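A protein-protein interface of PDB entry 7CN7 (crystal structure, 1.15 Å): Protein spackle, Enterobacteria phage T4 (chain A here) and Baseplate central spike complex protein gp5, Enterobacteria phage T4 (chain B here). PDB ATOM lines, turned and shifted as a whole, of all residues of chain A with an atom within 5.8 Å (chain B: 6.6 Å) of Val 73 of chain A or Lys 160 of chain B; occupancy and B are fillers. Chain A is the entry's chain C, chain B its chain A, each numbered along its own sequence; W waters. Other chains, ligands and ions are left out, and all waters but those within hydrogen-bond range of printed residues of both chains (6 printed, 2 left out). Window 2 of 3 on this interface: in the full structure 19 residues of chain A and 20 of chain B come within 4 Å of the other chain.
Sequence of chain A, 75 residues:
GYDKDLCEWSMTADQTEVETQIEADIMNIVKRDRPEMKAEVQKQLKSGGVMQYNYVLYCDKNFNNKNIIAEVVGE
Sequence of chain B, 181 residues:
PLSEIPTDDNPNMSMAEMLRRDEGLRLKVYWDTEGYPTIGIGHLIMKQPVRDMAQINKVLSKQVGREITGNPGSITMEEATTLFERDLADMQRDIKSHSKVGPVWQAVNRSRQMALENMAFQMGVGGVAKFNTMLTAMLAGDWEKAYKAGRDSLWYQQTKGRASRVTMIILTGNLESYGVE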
ATOM      1  N   ARG A  34       9.136  -0.708  15.827  1.00  0.00           N
ATOM      2  CA  ARG A  34       9.431   0.459  16.672  1.00  0.00           C
ATOM      3  C   ARG A  34       8.120   1.079  17.120  1.00  0.00           C
ATOM      4  O   ARG A  34       7.771   2.198  16.728  1.00  0.00           O
ATOM      5  CB  ARG A  34      10.332   1.457  15.949  1.00  0.00           C
ATOM      6  CG  ARG A  34      11.749   0.924  15.682  1.00  0.00           C
ATOM      7  CD  ARG A  34      12.723   2.054  15.391  1.00  0.00           C
ATOM      8  NE  ARG A  34      12.774   2.333  13.975  1.00  0.00           N
ATOM      9  CZ  ARG A  34      13.357   3.392  13.426  1.00  0.00           C
ATOM     10  NH1 ARG A  34      13.951   4.313  14.176  1.00  0.00           N
ATOM     11  NH2 ARG A  34      13.380   3.499  12.120  1.00  0.00           N
ATOM     12  N   MET A  37       7.205   4.782  18.005  1.00  0.00           N
ATOM     13  CA  MET A  37       7.190   5.841  17.005  1.00  0.00           C
ATOM     14  C   MET A  37       5.823   6.053  16.365  1.00  0.00           C
ATOM     15  O   MET A  37       5.713   6.870  15.445  1.00  0.00           O
ATOM     16  CB  MET A  37       8.272   5.569  15.949  1.00  0.00           C
ATOM     17  CG  MET A  37       9.680   5.533  16.553  1.00  0.00           C
ATOM     18  SD  MET A  37      11.000   5.265  15.372  1.00  0.00           S
ATOM     19  CE  MET A  37      10.954   6.835  14.572  1.00  0.00           C
ATOM     20  N   GLU A  40       4.465   9.741  16.116  1.00  0.00           N
ATOM     21  CA  GLU A  40       5.367  10.551  15.300  1.00  0.00           C
ATOM     22  C   GLU A  40       5.215  10.223  13.818  1.00  0.00           C
ATOM     23  O   GLU A  40       5.212  11.125  12.974  1.00  0.00           O
ATOM     24  CB  GLU A  40       6.809  10.335  15.771  1.00  0.00           C
ATOM     25  CG  GLU A  40       7.845  11.118  15.010  1.00  0.00           C
ATOM     26  CD  GLU A  40       9.247  11.025  15.589  1.00  0.00           C
ATOM     27  OE1 GLU A  40       9.492  10.336  16.612  1.00  0.00           O
ATOM     28  OE2 GLU A  40      10.138  11.659  14.992  1.00  0.00           O
ATOM     29  N   VAL A  41       5.125   8.935  13.485  1.00  0.00           N
ATOM     30  CA  VAL A  41       4.881   8.532  12.110  1.00  0.00           C
ATOM     31  C   VAL A  41       3.552   9.093  11.629  1.00  0.00           C
ATOM     32  O   VAL A  41       3.454   9.629  10.520  1.00  0.00           O
ATOM     33  CB  VAL A  41       4.965   7.008  11.973  1.00  0.00           C
ATOM     34  CG1 VAL A  41       4.498   6.562  10.621  1.00  0.00           C
ATOM     35  CG2 VAL A  41       6.390   6.539  12.231  1.00  0.00           C
ATOM     36  N   GLN A  44       3.791  12.719  10.657  1.00  0.00           N
ATOM     37  CA  GLN A  44       4.478  12.950   9.387  1.00  0.00           C
ATOM     38  C   GLN A  44       3.662  12.477   8.186  1.00  0.00           C
ATOM     39  O   GLN A  44       3.756  13.073   7.108  1.00  0.00           O
ATOM     40  CB  GLN A  44       5.842  12.264   9.396  1.00  0.00           C
ATOM     41  CG  GLN A  44       6.884  13.013  10.190  1.00  0.00           C
ATOM     42  CD  GLN A  44       7.149  14.385   9.615  1.00  0.00           C
ATOM     43  OE1 GLN A  44       7.331  14.543   8.403  1.00  0.00           O
ATOM     44  NE2 GLN A  44       7.163  15.387  10.464  1.00  0.00           N
ATOM     45  N   ILE A  68      10.754   1.607   5.953  1.00  0.00           N
ATOM     46  CA  ILE A  68       9.749   2.638   5.736  1.00  0.00           C
ATOM     47  C   ILE A  68       9.646   3.580   6.923  1.00  0.00           C
ATOM     48  O   ILE A  68       9.261   4.732   6.754  1.00  0.00           O
ATOM     49  CB  ILE A  68       8.393   2.027   5.359  1.00  0.00           C
ATOM     50  CG1 ILE A  68       7.531   3.077   4.640  1.00  0.00           C
ATOM     51  CG2 ILE A  68       7.672   1.432   6.578  1.00  0.00           C
ATOM     52  CD1 ILE A  68       8.047   3.459   3.250  1.00  0.00           C
ATOM     53  N   ILE A  69       9.955   3.127   8.142  1.00  0.00           N
ATOM     54  CA  ILE A  69       9.847   4.023   9.284  1.00  0.00           C
ATOM     55  C   ILE A  69      10.813   5.184   9.110  1.00  0.00           C
ATOM     56  O   ILE A  69      10.422   6.356   9.196  1.00  0.00           O
ATOM     57  CB  ILE A  69      10.081   3.277  10.617  1.00  0.00           C
ATOM     58  CG1 ILE A  69       9.172   2.054  10.750  1.00  0.00           C
ATOM     59  CG2 ILE A  69       9.880   4.276  11.763  1.00  0.00           C
ATOM     60  CD1 ILE A  69       9.391   1.291  12.067  1.00  0.00           C
ATOM     61  N   ALA A  70      12.080   4.866   8.832  1.00  0.00           N
ATOM     62  CA  ALA A  70      13.069   5.904   8.563  1.00  0.00           C
ATOM     63  C   ALA A  70      12.704   6.717   7.329  1.00  0.00           C
ATOM     64  O   ALA A  70      12.977   7.922   7.266  1.00  0.00           O
ATOM     65  CB  ALA A  70      14.450   5.288   8.402  1.00  0.00           C
ATOM     66  N   GLU A  71      12.097   6.081   6.322  1.00  0.00           N
ATOM     67  CA  GLU A  71      11.688   6.808   5.135  1.00  0.00           C
ATOM     68  C   GLU A  71      10.733   7.928   5.492  1.00  0.00           C
ATOM     69  O   GLU A  71      10.796   9.015   4.910  1.00  0.00           O
ATOM     70  CB  GLU A  71      11.043   5.851   4.131  1.00  0.00           C
ATOM     71  CG  GLU A  71      10.956   6.407   2.723  1.00  0.00           C
ATOM     72  CD  GLU A  71      12.271   6.425   1.965  1.00  0.00           C
ATOM     73  OE1 GLU A  71      13.309   6.032   2.531  1.00  0.00           O
ATOM     74  OE2 GLU A  71      12.235   6.850   0.786  1.00  0.00           O
ATOM     75  N   VAL A  72       9.817   7.680   6.423  1.00  0.00           N
ATOM     76  CA  VAL A  72       8.796   8.650   6.802  1.00  0.00           C
ATOM     77  C   VAL A  72       9.336   9.683   7.775  1.00  0.00           C
ATOM     78  O   VAL A  72       9.037  10.873   7.656  1.00  0.00           O
ATOM     79  CB  VAL A  72       7.559   7.938   7.374  1.00  0.00           C
ATOM     80  CG1 VAL A  72       6.553   8.964   7.905  1.00  0.00           C
ATOM     81  CG2 VAL A  72       6.921   7.028   6.309  1.00  0.00           C
ATOM     82  N   VAL A  73      10.078   9.256   8.800  1.00  0.00           N
ATOM     83  CA  VAL A  73      10.435  10.163   9.884  1.00  0.00           C
ATOM     84  C   VAL A  73      11.872  10.648   9.855  1.00  0.00           C
ATOM     85  O   VAL A  73      12.174  11.654  10.506  1.00  0.00           O
ATOM     86  CB  VAL A  73      10.094   9.604  11.274  1.00  0.00           C
ATOM     87  CG1 VAL A  73       8.647   9.266  11.378  1.00  0.00           C
ATOM     88  CG2 VAL A  73      10.934   8.436  11.630  1.00  0.00           C
ATOM     89  N   GLY A  74      12.770   9.960   9.158  1.00  0.00           N
ATOM     90  CA  GLY A  74      14.140  10.415   9.045  1.00  0.00           C
ATOM     91  C   GLY A  74      15.095   9.848  10.065  1.00  0.00           C
ATOM     92  O   GLY A  74      16.225  10.359  10.171  1.00  0.00           O
ATOM     93  N   GLU A  75      14.704   8.791  10.789  1.00  0.00           N
ATOM     94  CA  GLU A  75      15.648   8.167  11.729  1.00  0.00           C
ATOM     95  C   GLU A  75      15.184   6.737  11.998  1.00  0.00           C
ATOM     96  O   GLU A  75      15.945   5.931  12.567  1.00  0.00           O
ATOM     97  CB  GLU A  75      15.865   8.930  13.024  1.00  0.00           C
ATOM     98  CG  GLU A  75      14.708   8.859  13.970  1.00  0.00           C
ATOM     99  CD  GLU A  75      15.034   9.403  15.367  1.00  0.00           C
ATOM    100  OE1 GLU A  75      16.218   9.687  15.669  1.00  0.00           O
ATOM    101  OE2 GLU A  75      14.099   9.539  16.175  1.00  0.00           O
ATOM    102  OXT GLU A  75      14.045   6.404  11.672  1.00  0.00           O
ATOM    103  N   ARG B 151      17.683  21.862   7.885  1.00  0.00           N
ATOM    104  CA  ARG B 151      16.789  21.252   8.861  1.00  0.00           C
ATOM    105  C   ARG B 151      16.030  22.281   9.684  1.00  0.00           C
ATOM    106  O   ARG B 151      15.027  21.932  10.308  1.00  0.00           O
ATOM    107  CB  ARG B 151      17.548  20.253   9.735  1.00  0.00           C
ATOM    108  CG  ARG B 151      18.068  19.074   8.937  1.00  0.00           C
ATOM    109  CD  ARG B 151      18.480  17.910   9.822  1.00  0.00           C
ATOM    110  NE  ARG B 151      18.779  16.754   8.989  1.00  0.00           N
ATOM    111  CZ  ARG B 151      18.808  15.494   9.405  1.00  0.00           C
ATOM    112  NH1 ARG B 151      18.562  15.185  10.675  1.00  0.00           N
ATOM    113  NH2 ARG B 151      19.086  14.544   8.529  1.00  0.00           N
ATOM    114  N   TRP B 155       9.996  22.975   5.643  1.00  0.00           N
ATOM    115  CA  TRP B 155      10.176  21.785   4.812  1.00  0.00           C
ATOM    116  C   TRP B 155      10.577  20.578   5.650  1.00  0.00           C
ATOM    117  O   TRP B 155       9.996  19.491   5.522  1.00  0.00           O
ATOM    118  CB  TRP B 155      11.251  22.109   3.789  1.00  0.00           C
ATOM    119  CG  TRP B 155      11.810  20.992   2.991  1.00  0.00           C
ATOM    120  CD1 TRP B 155      11.152  20.193   2.103  1.00  0.00           C
ATOM    121  CD2 TRP B 155      13.186  20.600   2.943  1.00  0.00           C
ATOM    122  NE1 TRP B 155      12.024  19.309   1.523  1.00  0.00           N
ATOM    123  CE2 TRP B 155      13.286  19.549   2.009  1.00  0.00           C
ATOM    124  CE3 TRP B 155      14.340  21.030   3.615  1.00  0.00           C
ATOM    125  CZ2 TRP B 155      14.498  18.928   1.704  1.00  0.00           C
ATOM    126  CZ3 TRP B 155      15.535  20.427   3.314  1.00  0.00           C
ATOM    127  CH2 TRP B 155      15.613  19.383   2.366  1.00  0.00           C
ATOM    128  N   TYR B 156      11.570  20.758   6.525  1.00  0.00           N
ATOM    129  CA  TYR B 156      12.011  19.660   7.369  1.00  0.00           C
ATOM    130  C   TYR B 156      10.913  19.240   8.343  1.00  0.00           C
ATOM    131  O   TYR B 156      10.757  18.055   8.642  1.00  0.00           O
ATOM    132  CB  TYR B 156      13.291  20.069   8.101  1.00  0.00           C
ATOM    133  CG  TYR B 156      13.774  19.051   9.098  1.00  0.00           C
ATOM    134  CD1 TYR B 156      14.557  17.969   8.721  1.00  0.00           C
ATOM    135  CD2 TYR B 156      13.458  19.187  10.438  1.00  0.00           C
ATOM    136  CE1 TYR B 156      15.016  17.035   9.655  1.00  0.00           C
ATOM    137  CE2 TYR B 156      13.896  18.273  11.367  1.00  0.00           C
ATOM    138  CZ  TYR B 156      14.677  17.204  10.981  1.00  0.00           C
ATOM    139  OH  TYR B 156      15.081  16.311  11.955  1.00  0.00           O
ATOM    140  N   GLN B 157      10.146  20.193   8.872  1.00  0.00           N
ATOM    141  CA  GLN B 157       9.113  19.796   9.818  1.00  0.00           C
ATOM    142  C   GLN B 157       7.959  19.083   9.133  1.00  0.00           C
ATOM    143  O   GLN B 157       7.361  18.183   9.731  1.00  0.00           O
ATOM    144  CB  GLN B 157       8.611  20.996  10.606  1.00  0.00           C
ATOM    145  CG  GLN B 157       9.630  21.514  11.631  1.00  0.00           C
ATOM    146  CD  GLN B 157      10.079  20.456  12.657  1.00  0.00           C
ATOM    147  OE1 GLN B 157       9.309  19.577  13.059  1.00  0.00           O
ATOM    148  NE2 GLN B 157      11.334  20.555  13.087  1.00  0.00           N
ATOM    149  N   GLN B 158       7.634  19.455   7.897  1.00  0.00           N
ATOM    150  CA  GLN B 158       6.465  18.906   7.227  1.00  0.00           C
ATOM    151  C   GLN B 158       6.730  17.620   6.469  1.00  0.00           C
ATOM    152  O   GLN B 158       5.862  16.735   6.445  1.00  0.00           O
ATOM    153  CB  GLN B 158       5.854  19.962   6.308  1.00  0.00           C
ATOM    154  CG  GLN B 158       5.343  21.170   7.076  1.00  0.00           C
ATOM    155  CD  GLN B 158       4.437  22.071   6.275  1.00  0.00           C
ATOM    156  OE1 GLN B 158       4.557  22.169   5.063  1.00  0.00           O
ATOM    157  NE2 GLN B 158       3.524  22.751   6.966  1.00  0.00           N
ATOM    158  N   THR B 159       7.883  17.521   5.812  1.00  0.00           N
ATOM    159  CA  THR B 159       8.301  16.318   5.113  1.00  0.00           C
ATOM    160  C   THR B 159       9.655  15.896   5.657  1.00  0.00           C
ATOM    161  O   THR B 159      10.679  16.013   4.985  1.00  0.00           O
ATOM    162  CB  THR B 159       8.327  16.520   3.575  1.00  0.00           C
ATOM    163  OG1 THR B 159       9.079  17.679   3.202  1.00  0.00           O
ATOM    164  CG2 THR B 159       6.933  16.673   3.024  1.00  0.00           C
ATOM    165  N   LYS B 160       9.656  15.426   6.903  1.00  0.00           N
ATOM    166  CA  LYS B 160      10.892  15.228   7.646  1.00  0.00           C
ATOM    167  C   LYS B 160      11.716  14.076   7.096  1.00  0.00           C
ATOM    168  O   LYS B 160      12.940  14.139   7.116  1.00  0.00           O
ATOM    169  CB  LYS B 160      10.571  15.010   9.122  1.00  0.00           C
ATOM    170  CG  LYS B 160      11.804  15.069  10.000  1.00  0.00           C
ATOM    171  CD  LYS B 160      11.481  14.980  11.474  1.00  0.00           C
ATOM    172  CE  LYS B 160      10.782  16.218  11.942  1.00  0.00           C
ATOM    173  NZ  LYS B 160      10.505  16.111  13.387  1.00  0.00           N
ATOM    174  N   GLY B 161      11.082  13.002   6.635  1.00  0.00           N
ATOM    175  CA  GLY B 161      11.860  11.885   6.138  1.00  0.00           C
ATOM    176  C   GLY B 161      12.675  12.270   4.921  1.00  0.00           C
ATOM    177  O   GLY B 161      13.900  12.094   4.871  1.00  0.00           O
ATOM    178  N   ARG B 162      12.001  12.840   3.931  1.00  0.00           N
ATOM    179  CA  ARG B 162      12.669  13.287   2.720  1.00  0.00           C
ATOM    180  C   ARG B 162      13.706  14.353   3.030  1.00  0.00           C
ATOM    181  O   ARG B 162      14.834  14.291   2.544  1.00  0.00           O
ATOM    182  CB  ARG B 162      11.624  13.810   1.738  1.00  0.00           C
ATOM    183  CG  ARG B 162      12.190  14.169   0.367  1.00  0.00           C
ATOM    184  CD  ARG B 162      11.053  14.492  -0.564  1.00  0.00           C
ATOM    185  NE  ARG B 162      11.511  14.818  -1.918  1.00  0.00           N
ATOM    186  CZ  ARG B 162      10.708  15.085  -2.930  1.00  0.00           C
ATOM    187  NH1 ARG B 162       9.407  15.043  -2.766  1.00  0.00           N
ATOM    188  NH2 ARG B 162      11.214  15.389  -4.118  1.00  0.00           N
ATOM    189  N   ALA B 163      13.344  15.339   3.846  1.00  0.00           N
ATOM    190  CA  ALA B 163      14.298  16.396   4.168  1.00  0.00           C
ATOM    191  C   ALA B 163      15.505  15.847   4.913  1.00  0.00           C
ATOM    192  O   ALA B 163      16.612  16.369   4.772  1.00  0.00           O
ATOM    193  CB  ALA B 163      13.634  17.484   4.997  1.00  0.00           C
ATOM    194  N   SER B 164      15.306  14.812   5.729  1.00  0.00           N
ATOM    195  CA  SER B 164      16.422  14.206   6.440  1.00  0.00           C
ATOM    196  C   SER B 164      17.409  13.574   5.471  1.00  0.00           C
ATOM    197  O   SER B 164      18.622  13.799   5.572  1.00  0.00           O
ATOM    198  CB  SER B 164      15.930  13.166   7.441  1.00  0.00           C
ATOM    199  OG  SER B 164      15.249  13.792   8.514  1.00  0.00           O
ATOM    200  N   ARG B 165      16.922  12.745   4.545  1.00  0.00           N
ATOM    201  CA  ARG B 165      17.851  12.096   3.625  1.00  0.00           C
ATOM    202  C   ARG B 165      18.471  13.090   2.642  1.00  0.00           C
ATOM    203  O   ARG B 165      19.642  12.937   2.278  1.00  0.00           O
ATOM    204  CB  ARG B 165      17.237  10.861   2.967  1.00  0.00           C
ATOM    205  CG  ARG B 165      15.935  11.009   2.289  1.00  0.00           C
ATOM    206  CD  ARG B 165      15.446   9.626   1.701  1.00  0.00           C
ATOM    207  NE  ARG B 165      14.138   9.835   1.137  1.00  0.00           N
ATOM    208  CZ  ARG B 165      13.002   9.834   1.838  1.00  0.00           C
ATOM    209  NH1 ARG B 165      12.971   9.548   3.127  1.00  0.00           N
ATOM    210  NH2 ARG B 165      11.880  10.117   1.218  1.00  0.00           N
HETATM  211  O   HOH W   1       9.212  13.524  13.550  1.00  0.00           O
HETATM  212  O   HOH W   2       4.673  17.572  11.231  1.00  0.00           O
HETATM  213  O   HOH W   3       9.778   7.774  -0.067  1.00  0.00           O
HETATM  214  O   HOH W   4      18.992  11.624   9.024  1.00  0.00           O
HETATM  215  O   HOH W   5       7.732  12.786   6.322  1.00  0.00           O
HETATM  216  O   HOH W   6      14.810   8.837   5.338  1.00  0.00           O
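The side-chain amide oxygen (OE1) of Gln 44 of chain A lies close to the backbone carbonyl oxygen (O) of Gln 158 of chain B (3.3 Å).
The backbone carbonyl oxygen (O) of Val 72 of chain A is in hydrogen-bond range of the backbone NH (N) of Gly 161 of chain B, at 3.1 Å.
The side-chain amide oxygen (OE1) of Gln 44 of chain A is in hydrogen-bond range of the backbone NH (N) of Lys 160 of chain B, 2.9 Å away.
NH2 of Arg 165 of chain B is in salt-bridge range of OE2 of Glu 71 of chain A (3.3 Å).
O of Gln 157 of chain B is in hydrogen-bond range of NE2 of Gln 44 of chain A (2.9 Å).
O of Ser 164 of chain B sits at hydrogen-bond distance from NH2 of Arg 151 of chain B (3.1 Å).
The backbone carbonyl oxygen (O) of Trp 155 of chain B lies within hydrogen-bond range of the side-chain hydroxyl (OG1) of Thr 159 of chain B, 3.1 Å away.
O of Lys 160 of chain B is in hydrogen-bond range of OG of Ser 164 of chain B, 2.7 Å away.
NH1 of Arg 165 of chain B lies within hydrogen-bond range of O of Gly 161 of chain B (3.2 Å).
Among the printed residues, pairs that only touch across the chains: Gln 44 of chain A with Thr 159 of chain B (3.8 Å), Glu 71 of chain A with Gly 161 of chain B (3.3 Å), Val 73 of chain A with Lys 160 of chain B (3.5 Å), Val 73 of chain A with Gly 161 of chain B (3.9 Å), Gly 74 of chain A with Gly 161 of chain B (3.7 Å) and Gly 74 of chain A with Ser 164 of chain B (3.6 Å).
Met 37 of chain A touches none of the printed residues of chain B.
Val 73 of chain A touches just these residues of chain B: Lys 160 and Gly 161.
Printed residues of chain B within 4 Å of Gly 74 of chain A: Gly 161 and Ser 164.
Of the printed residues of chain A, Gln 158 of chain B touches Gln 44.
Lys 160 of chain B touches just these residues of chain A: Gln 44 and Val 73.
Of the printed residues of chain A, Gly 161 of chain B touches Glu 71, Val 72, Val 73 and Gly 74.
Printed residues of chain A within 4 Å of Arg 165 of chain B: Glu 71 (2.9 Å).
The nearest residue of chain B that does not touch Val 73 of chain A is Ser 164 of chain B (4.2 Å).
The nearest residue of chain A that does not touch Lys 160 of chain B is Val 72 of chain A (4.2 Å).
The nearest printed residue of chain A that does not touch Gln 157 of chain B is Val 72 of chain A (7.8 Å).
Printed residues of chain B that touch a printed residue of chain A: Gln 157, Gln 158, Thr 159, Lys 160, Gly 161, Ser 164 and Arg 165.
Among the printed residues, 11 pairs touch across the chains.
Among the printed residues, Asp or Glu carboxylates within 4 Å of a Lys or Arg side-chain nitrogen of the other chain: Glu 71 of chain A with Arg 165 of chain B.
Water W1 lies within hydrogen-bond range of OE2 of Glu 40 of chain A (2.5 Å) and NZ of Lys 160 of chain B (2.9 Å).
Water W5 lies within hydrogen-bond range of O of Val 72 of chain A (2.7 Å), OE1 of Gln 44 of chain A (2.8 Å), N of Lys 160 of chain B (3.3 Å) and N of Gly 161 of chain B (3.4 Å).
Water W3 bridges the side-chain carboxylate of Glu 71 of chain A and the guanidinium group of Arg 165 of chain B.
Water W6 lies within hydrogen-bond range of the backbone carbonyl oxygen of Ala 70 of chain A (2.8 Å), the guanidinium group of Arg 165 of chain B (3.0 Å) and the backbone carbonyl oxygen of Gly 161 of chain B (3.4 Å).
Water W4 lies within hydrogen-bond range of the guanidinium group of Arg 151 of chain B (3.0 Å) and the backbone carbonyl oxygen of Gly 74 of chain A (3.3 Å).
Water W2 lies within hydrogen-bond range of O of Gln 157 of chain B (3.1 Å) and NE2 of Gln 44 of chain A (3.4 Å).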
